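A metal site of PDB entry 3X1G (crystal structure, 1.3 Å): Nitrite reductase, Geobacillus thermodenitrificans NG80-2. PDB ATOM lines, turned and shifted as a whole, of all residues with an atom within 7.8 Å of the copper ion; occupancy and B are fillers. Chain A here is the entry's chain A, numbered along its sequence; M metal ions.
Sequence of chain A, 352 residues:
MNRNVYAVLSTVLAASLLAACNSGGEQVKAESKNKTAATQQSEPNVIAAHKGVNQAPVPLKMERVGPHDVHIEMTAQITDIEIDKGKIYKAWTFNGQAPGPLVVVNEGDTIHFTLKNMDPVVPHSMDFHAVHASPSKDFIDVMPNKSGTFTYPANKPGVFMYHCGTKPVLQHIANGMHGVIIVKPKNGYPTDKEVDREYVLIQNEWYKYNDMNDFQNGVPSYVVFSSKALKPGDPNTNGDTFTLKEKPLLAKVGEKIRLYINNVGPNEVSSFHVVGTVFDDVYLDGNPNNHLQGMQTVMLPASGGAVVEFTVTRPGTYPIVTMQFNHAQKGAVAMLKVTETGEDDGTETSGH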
ATOM      1  N   ALA A  76      34.602  10.816  17.075  1.00  0.00           N
ATOM      2  CA  ALA A  76      33.158  10.867  17.183  1.00  0.00           C
ATOM      3  C   ALA A  76      32.745  12.229  16.668  1.00  0.00           C
ATOM      4  O   ALA A  76      33.298  13.259  17.111  1.00  0.00           O
ATOM      5  CB  ALA A  76      32.715  10.684  18.646  1.00  0.00           C
ATOM      6  N   TRP A  92      24.966  10.759  14.444  1.00  0.00           N
ATOM      7  CA  TRP A  92      26.078  10.622  15.415  1.00  0.00           C
ATOM      8  C   TRP A  92      26.949   9.520  14.871  1.00  0.00           C
ATOM      9  O   TRP A  92      26.462   8.437  14.583  1.00  0.00           O
ATOM     10  CB  TRP A  92      25.568  10.258  16.802  1.00  0.00           C
ATOM     11  CG  TRP A  92      24.612  11.226  17.425  1.00  0.00           C
ATOM     12  CD1 TRP A  92      23.968  12.300  16.888  1.00  0.00           C
ATOM     13  CD2 TRP A  92      24.181  11.137  18.780  1.00  0.00           C
ATOM     14  NE1 TRP A  92      23.186  12.924  17.841  1.00  0.00           N
ATOM     15  CE2 TRP A  92      23.277  12.202  19.016  1.00  0.00           C
ATOM     16  CE3 TRP A  92      24.420  10.227  19.805  1.00  0.00           C
ATOM     17  CZ2 TRP A  92      22.668  12.399  20.267  1.00  0.00           C
ATOM     18  CZ3 TRP A  92      23.771  10.405  21.016  1.00  0.00           C
ATOM     19  CH2 TRP A  92      22.910  11.484  21.250  1.00  0.00           C
ATOM     20  N   THR A  93      28.230   9.815  14.627  1.00  0.00           N
ATOM     21  CA  THR A  93      29.048   8.928  13.852  1.00  0.00           C
ATOM     22  C   THR A  93      30.466   8.753  14.440  1.00  0.00           C
ATOM     23  O   THR A  93      30.943   9.615  15.213  1.00  0.00           O
ATOM     24  CB  THR A  93      29.266   9.477  12.413  1.00  0.00           C
ATOM     25  OG1 THR A  93      30.194  10.574  12.390  1.00  0.00           O
ATOM     26  CG2 THR A  93      27.983   9.872  11.755  1.00  0.00           C
ATOM     27  N   PHE A  94      31.107   7.716  13.966  1.00  0.00           N
ATOM     28  CA  PHE A  94      32.552   7.630  13.924  1.00  0.00           C
ATOM     29  C   PHE A  94      33.033   8.098  12.583  1.00  0.00           C
ATOM     30  O   PHE A  94      32.650   7.567  11.539  1.00  0.00           O
ATOM     31  CB  PHE A  94      33.047   6.221  14.217  1.00  0.00           C
ATOM     32  CG  PHE A  94      32.626   5.682  15.571  1.00  0.00           C
ATOM     33  CD1 PHE A  94      33.227   6.171  16.731  1.00  0.00           C
ATOM     34  CD2 PHE A  94      31.567   4.778  15.717  1.00  0.00           C
ATOM     35  CE1 PHE A  94      32.912   5.625  17.956  1.00  0.00           C
ATOM     36  CE2 PHE A  94      31.248   4.265  16.980  1.00  0.00           C
ATOM     37  CZ  PHE A  94      31.867   4.734  18.097  1.00  0.00           C
ATOM     38  N   LEU A 115      40.055   7.639  20.638  1.00  0.00           N
ATOM     39  CA  LEU A 115      38.837   8.276  20.215  1.00  0.00           C
ATOM     40  C   LEU A 115      38.997   9.755  20.496  1.00  0.00           C
ATOM     41  O   LEU A 115      39.191  10.163  21.644  1.00  0.00           O
ATOM     42  CB  LEU A 115      37.597   7.725  20.946  1.00  0.00           C
ATOM     43  CG  LEU A 115      36.255   8.302  20.499  1.00  0.00           C
ATOM     44  CD1 LEU A 115      35.964   7.964  19.045  1.00  0.00           C
ATOM     45  CD2 LEU A 115      35.158   7.781  21.419  1.00  0.00           C
ATOM     46  N   ASN A 117      36.829  13.002  20.488  1.00  0.00           N
ATOM     47  CA  ASN A 117      35.397  13.379  20.523  1.00  0.00           C
ATOM     48  C   ASN A 117      35.239  14.819  19.996  1.00  0.00           C
ATOM     49  O   ASN A 117      35.599  15.754  20.728  1.00  0.00           O
ATOM     50  CB  ASN A 117      34.797  13.211  21.878  1.00  0.00           C
ATOM     51  CG  ASN A 117      33.296  13.375  21.863  1.00  0.00           C
ATOM     52  OD1 ASN A 117      32.711  13.643  20.774  1.00  0.00           O
ATOM     53  ND2 ASN A 117      32.640  13.332  23.009  1.00  0.00           N
ATOM     54  N   ASP A 119      32.180  15.948  19.095  1.00  0.00           N
ATOM     55  CA  ASP A 119      30.851  16.389  19.419  1.00  0.00           C
ATOM     56  C   ASP A 119      30.960  17.532  20.469  1.00  0.00           C
ATOM     57  O   ASP A 119      31.665  17.365  21.444  1.00  0.00           O
ATOM     58  CB  ASP A 119      30.106  15.186  20.042  1.00  0.00           C
ATOM     59  CG  ASP A 119      28.622  15.411  20.233  1.00  0.00           C
ATOM     60  OD1 ASP A 119      28.202  16.552  20.680  1.00  0.00           O
ATOM     61  OD2 ASP A 119      27.785  14.513  20.012  1.00  0.00           O
ATOM     62  N   VAL A 122      27.927  16.049  23.581  1.00  0.00           N
ATOM     63  CA  VAL A 122      27.623  14.660  24.063  1.00  0.00           C
ATOM     64  C   VAL A 122      28.920  13.868  24.204  1.00  0.00           C
ATOM     65  O   VAL A 122      29.708  13.821  23.243  1.00  0.00           O
ATOM     66  CB  VAL A 122      26.604  13.925  23.120  1.00  0.00           C
ATOM     67  CG1 VAL A 122      26.151  12.663  23.780  1.00  0.00           C
ATOM     68  CG2 VAL A 122      25.428  14.828  22.779  1.00  0.00           C
ATOM     69  N   PRO A 123      29.114  13.179  25.349  1.00  0.00           N
ATOM     70  CA  PRO A 123      30.216  12.220  25.456  1.00  0.00           C
ATOM     71  C   PRO A 123      30.002  11.008  24.492  1.00  0.00           C
ATOM     72  O   PRO A 123      28.849  10.677  24.199  1.00  0.00           O
ATOM     73  CB  PRO A 123      30.205  11.739  26.928  1.00  0.00           C
ATOM     74  CG  PRO A 123      29.369  12.745  27.621  1.00  0.00           C
ATOM     75  CD  PRO A 123      28.360  13.253  26.589  1.00  0.00           C
ATOM     76  N   HIS A 124      31.094  10.375  24.116  1.00  0.00           N
ATOM     77  CA  HIS A 124      31.034   9.167  23.300  1.00  0.00           C
ATOM     78  C   HIS A 124      32.084   8.171  23.757  1.00  0.00           C
ATOM     79  O   HIS A 124      33.025   8.538  24.483  1.00  0.00           O
ATOM     80  CB  HIS A 124      31.141   9.466  21.794  1.00  0.00           C
ATOM     81  CG  HIS A 124      30.078  10.329  21.294  1.00  0.00           C
ATOM     82  ND1 HIS A 124      28.782   9.901  21.143  1.00  0.00           N
ATOM     83  CD2 HIS A 124      30.061  11.636  20.914  1.00  0.00           C
ATOM     84  CE1 HIS A 124      28.018  10.888  20.719  1.00  0.00           C
ATOM     85  NE2 HIS A 124      28.760  11.944  20.603  1.00  0.00           N
ATOM     86  N   SER A 125      32.012   6.939  23.278  1.00  0.00           N
ATOM     87  CA  SER A 125      32.876   5.863  23.729  1.00  0.00           C
ATOM     88  C   SER A 125      32.953   4.821  22.630  1.00  0.00           C
ATOM     89  O   SER A 125      32.278   4.984  21.566  1.00  0.00           O
ATOM     90  CB  SER A 125      32.380   5.222  25.000  1.00  0.00           C
ATOM     91  OG  SER A 125      31.052   4.712  24.815  1.00  0.00           O
ATOM     92  N   MET A 126      33.740   3.771  22.827  1.00  0.00           N
ATOM     93  CA  MET A 126      33.875   2.700  21.842  1.00  0.00           C
ATOM     94  C   MET A 126      33.921   1.340  22.554  1.00  0.00           C
ATOM     95  O   MET A 126      34.714   1.100  23.452  1.00  0.00           O
ATOM     96  CB  MET A 126      35.217   2.841  21.072  1.00  0.00           C
ATOM     97  CG  MET A 126      35.501   1.758  20.102  1.00  0.00           C
ATOM     98  SD  MET A 126      34.246   1.497  18.778  1.00  0.00           S
ATOM     99  CE  MET A 126      34.871   2.706  17.614  1.00  0.00           C
ATOM    100  N   ASP A 141      33.669   6.758  28.665  1.00  0.00           N
ATOM    101  CA  ASP A 141      33.385   7.955  27.898  1.00  0.00           C
ATOM    102  C   ASP A 141      34.591   8.853  27.694  1.00  0.00           C
ATOM    103  O   ASP A 141      35.449   8.997  28.582  1.00  0.00           O
ATOM    104  CB  ASP A 141      32.281   8.764  28.557  1.00  0.00           C
ATOM    105  CG  ASP A 141      30.908   8.130  28.470  1.00  0.00           C
ATOM    106  OD1 ASP A 141      30.702   7.124  27.687  1.00  0.00           O
ATOM    107  OD2 ASP A 141      30.020   8.473  29.286  1.00  0.00           O
ATOM    108  N   HIS A 163      30.601  -0.376  18.332  1.00  0.00           N
ATOM    109  CA  HIS A 163      29.597   0.687  18.489  1.00  0.00           C
ATOM    110  C   HIS A 163      29.928   1.547  19.725  1.00  0.00           C
ATOM    111  O   HIS A 163      30.625   1.102  20.641  1.00  0.00           O
ATOM    112  CB  HIS A 163      28.191   0.089  18.645  1.00  0.00           C
ATOM    113  CG  HIS A 163      28.040  -0.680  19.907  1.00  0.00           C
ATOM    114  ND1 HIS A 163      27.652  -0.099  21.098  1.00  0.00           N
ATOM    115  CD2 HIS A 163      28.301  -1.968  20.213  1.00  0.00           C
ATOM    116  CE1 HIS A 163      27.702  -1.005  22.097  1.00  0.00           C
ATOM    117  NE2 HIS A 163      28.105  -2.140  21.581  1.00  0.00           N
ATOM    118  N   CYS A 164      29.341   2.731  19.762  1.00  0.00           N
ATOM    119  CA  CYS A 164      29.426   3.581  20.979  1.00  0.00           C
ATOM    120  C   CYS A 164      28.794   2.853  22.118  1.00  0.00           C
ATOM    121  O   CYS A 164      27.700   2.284  21.974  1.00  0.00           O
ATOM    122  CB  CYS A 164      28.848   4.957  20.648  1.00  0.00           C
ATOM    123  SG  CYS A 164      28.862   6.053  22.019  1.00  0.00           S
ATOM    124  N   GLY A 165      29.393   3.004  23.309  1.00  0.00           N
ATOM    125  CA  GLY A 165      28.918   2.401  24.539  1.00  0.00           C
ATOM    126  C   GLY A 165      28.450   3.352  25.602  1.00  0.00           C
ATOM    127  O   GLY A 165      28.430   2.998  26.760  1.00  0.00           O
ATOM    128  N   THR A 166      28.034   4.561  25.178  1.00  0.00           N
ATOM    129  CA  THR A 166      27.637   5.592  26.141  1.00  0.00           C
ATOM    130  C   THR A 166      26.164   5.499  26.409  1.00  0.00           C
ATOM    131  O   THR A 166      25.350   5.388  25.496  1.00  0.00           O
ATOM    132  CB  THR A 166      28.021   6.951  25.518  1.00  0.00           C
ATOM    133  OG1 THR A 166      29.467   7.006  25.345  1.00  0.00           O
ATOM    134  CG2 THR A 166      27.583   8.131  26.412  1.00  0.00           C
ATOM    135  N   LYS A 167      25.789   5.612  27.674  1.00  0.00           N
ATOM    136  CA  LYS A 167      24.385   5.479  28.023  1.00  0.00           C
ATOM    137  C   LYS A 167      23.636   6.747  27.572  1.00  0.00           C
ATOM    138  O   LYS A 167      24.142   7.903  27.753  1.00  0.00           O
ATOM    139  CB  LYS A 167      24.239   5.404  29.553  1.00  0.00           C
ATOM    140  CG  LYS A 167      22.843   5.228  30.082  1.00  0.00           C
ATOM    141  CD  LYS A 167      22.782   5.177  31.630  1.00  0.00           C
ATOM    142  CE  LYS A 167      21.331   5.163  32.215  1.00  0.00           C
ATOM    143  NZ  LYS A 167      21.145   4.729  33.653  1.00  0.00           N
ATOM    144  N   PRO A 168      22.376   6.619  27.064  1.00  0.00           N
ATOM    145  CA  PRO A 168      21.710   5.376  26.685  1.00  0.00           C
ATOM    146  C   PRO A 168      22.319   4.796  25.386  1.00  0.00           C
ATOM    147  O   PRO A 168      22.310   5.483  24.341  1.00  0.00           O
ATOM    148  CB  PRO A 168      20.267   5.763  26.442  1.00  0.00           C
ATOM    149  CG  PRO A 168      20.162   7.201  26.805  1.00  0.00           C
ATOM    150  CD  PRO A 168      21.537   7.788  26.731  1.00  0.00           C
ATOM    151  N   VAL A 169      22.798   3.566  25.454  1.00  0.00           N
ATOM    152  CA  VAL A 169      23.476   2.981  24.284  1.00  0.00           C
ATOM    153  C   VAL A 169      22.551   2.879  23.097  1.00  0.00           C
ATOM    154  O   VAL A 169      22.971   3.139  21.973  1.00  0.00           O
ATOM    155  CB  VAL A 169      24.098   1.623  24.705  1.00  0.00           C
ATOM    156  CG1 VAL A 169      24.668   0.883  23.498  1.00  0.00           C
ATOM    157  CG2 VAL A 169      25.193   1.835  25.743  1.00  0.00           C
ATOM    158  N   GLN A 171      20.399   5.005  22.160  1.00  0.00           N
ATOM    159  CA  GLN A 171      20.413   6.307  21.492  1.00  0.00           C
ATOM    160  C   GLN A 171      21.628   6.463  20.616  1.00  0.00           C
ATOM    161  O   GLN A 171      21.549   6.955  19.487  1.00  0.00           O
ATOM    162  CB  GLN A 171      20.295   7.428  22.539  1.00  0.00           C
ATOM    163  CG  GLN A 171      20.172   8.800  21.929  1.00  0.00           C
ATOM    164  CD  GLN A 171      19.979   9.846  23.004  1.00  0.00           C
ATOM    165  OE1 GLN A 171      20.260   9.624  24.185  1.00  0.00           O
ATOM    166  NE2 GLN A 171      19.458  10.993  22.604  1.00  0.00           N
ATOM    167  N   HIS A 172      22.804   6.118  21.161  1.00  0.00           N
ATOM    168  CA  HIS A 172      24.044   6.307  20.441  1.00  0.00           C
ATOM    169  C   HIS A 172      24.120   5.391  19.203  1.00  0.00           C
ATOM    170  O   HIS A 172      24.512   5.827  18.128  1.00  0.00           O
ATOM    171  CB  HIS A 172      25.243   6.134  21.354  1.00  0.00           C
ATOM    172  CG  HIS A 172      25.379   7.255  22.338  1.00  0.00           C
ATOM    173  ND1 HIS A 172      26.401   8.167  22.189  1.00  0.00           N
ATOM    174  CD2 HIS A 172      24.618   7.622  23.399  1.00  0.00           C
ATOM    175  CE1 HIS A 172      26.267   9.086  23.161  1.00  0.00           C
ATOM    176  NE2 HIS A 172      25.209   8.736  23.896  1.00  0.00           N
ATOM    177  N   ILE A 173      23.704   4.113  19.367  1.00  0.00           N
ATOM    178  CA  ILE A 173      23.714   3.207  18.217  1.00  0.00           C
ATOM    179  C   ILE A 173      22.701   3.681  17.201  1.00  0.00           C
ATOM    180  O   ILE A 173      22.991   3.773  15.985  1.00  0.00           O
ATOM    181  CB  ILE A 173      23.453   1.758  18.612  1.00  0.00           C
ATOM    182  CG1 ILE A 173      24.525   1.221  19.579  1.00  0.00           C
ATOM    183  CG2 ILE A 173      23.407   0.864  17.381  1.00  0.00           C
ATOM    184  CD1 ILE A 173      24.277  -0.187  20.080  1.00  0.00           C
ATOM    185  N   ASN A 175      21.407   6.489  16.475  1.00  0.00           N
ATOM    186  CA  ASN A 175      21.786   7.698  15.788  1.00  0.00           C
ATOM    187  C   ASN A 175      22.963   7.523  14.827  1.00  0.00           C
ATOM    188  O   ASN A 175      23.259   8.466  14.069  1.00  0.00           O
ATOM    189  CB  ASN A 175      22.071   8.839  16.753  1.00  0.00           C
ATOM    190  CG  ASN A 175      20.815   9.476  17.294  1.00  0.00           C
ATOM    191  OD1 ASN A 175      19.792   9.607  16.623  1.00  0.00           O
ATOM    192  ND2 ASN A 175      20.917   9.965  18.528  1.00  0.00           N
ATOM    193  N   GLY A 176      23.602   6.360  14.795  1.00  0.00           N
ATOM    194  CA  GLY A 176      24.578   6.024  13.800  1.00  0.00           C
ATOM    195  C   GLY A 176      25.918   5.471  14.266  1.00  0.00           C
ATOM    196  O   GLY A 176      26.762   5.201  13.410  1.00  0.00           O
ATOM    197  N   MET A 177      26.111   5.301  15.587  1.00  0.00           N
ATOM    198  CA  MET A 177      27.479   4.969  16.050  1.00  0.00           C
ATOM    199  C   MET A 177      27.666   3.453  16.174  1.00  0.00           C
ATOM    200  O   MET A 177      27.665   2.839  17.234  1.00  0.00           O
ATOM    201  CB  MET A 177      27.708   5.632  17.429  1.00  0.00           C
ATOM    202  CG  MET A 177      27.524   7.146  17.346  1.00  0.00           C
ATOM    203  SD  MET A 177      28.188   8.118  18.682  1.00  0.00           S
ATOM    204  CE  MET A 177      29.920   8.067  18.324  1.00  0.00           C
HETATM  205 CU    CU M   1      28.158   7.956  21.273  1.00  0.00          CU
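Within 4 Å of the copper ion: His 124, Cys 164, His 172 and Met 177.
The copper ion is bound by ND1 of His 172 (2.0 Å), ND1 of His 124 (2.0 Å), SG of Cys 164 (2.2 Å) and SD of Met 177 (2.6 Å).
NE2 of His 124 lies close to O of Val 122, 3.4 Å away.
The backbone NH (N) of Ser 125 sits close to the side-chain sulfur (SG) of Cys 164 (3.5 Å).
O of Trp 92 sits close to N of Met 177 (3.3 Å).
The side-chain hydroxyl (OG1) of Thr 166 lies close to the side-chain sulfur (SG) of Cys 164, 3.5 Å away.
NE2 of His 124 is in hydrogen-bond range of OD2 of Asp 119.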
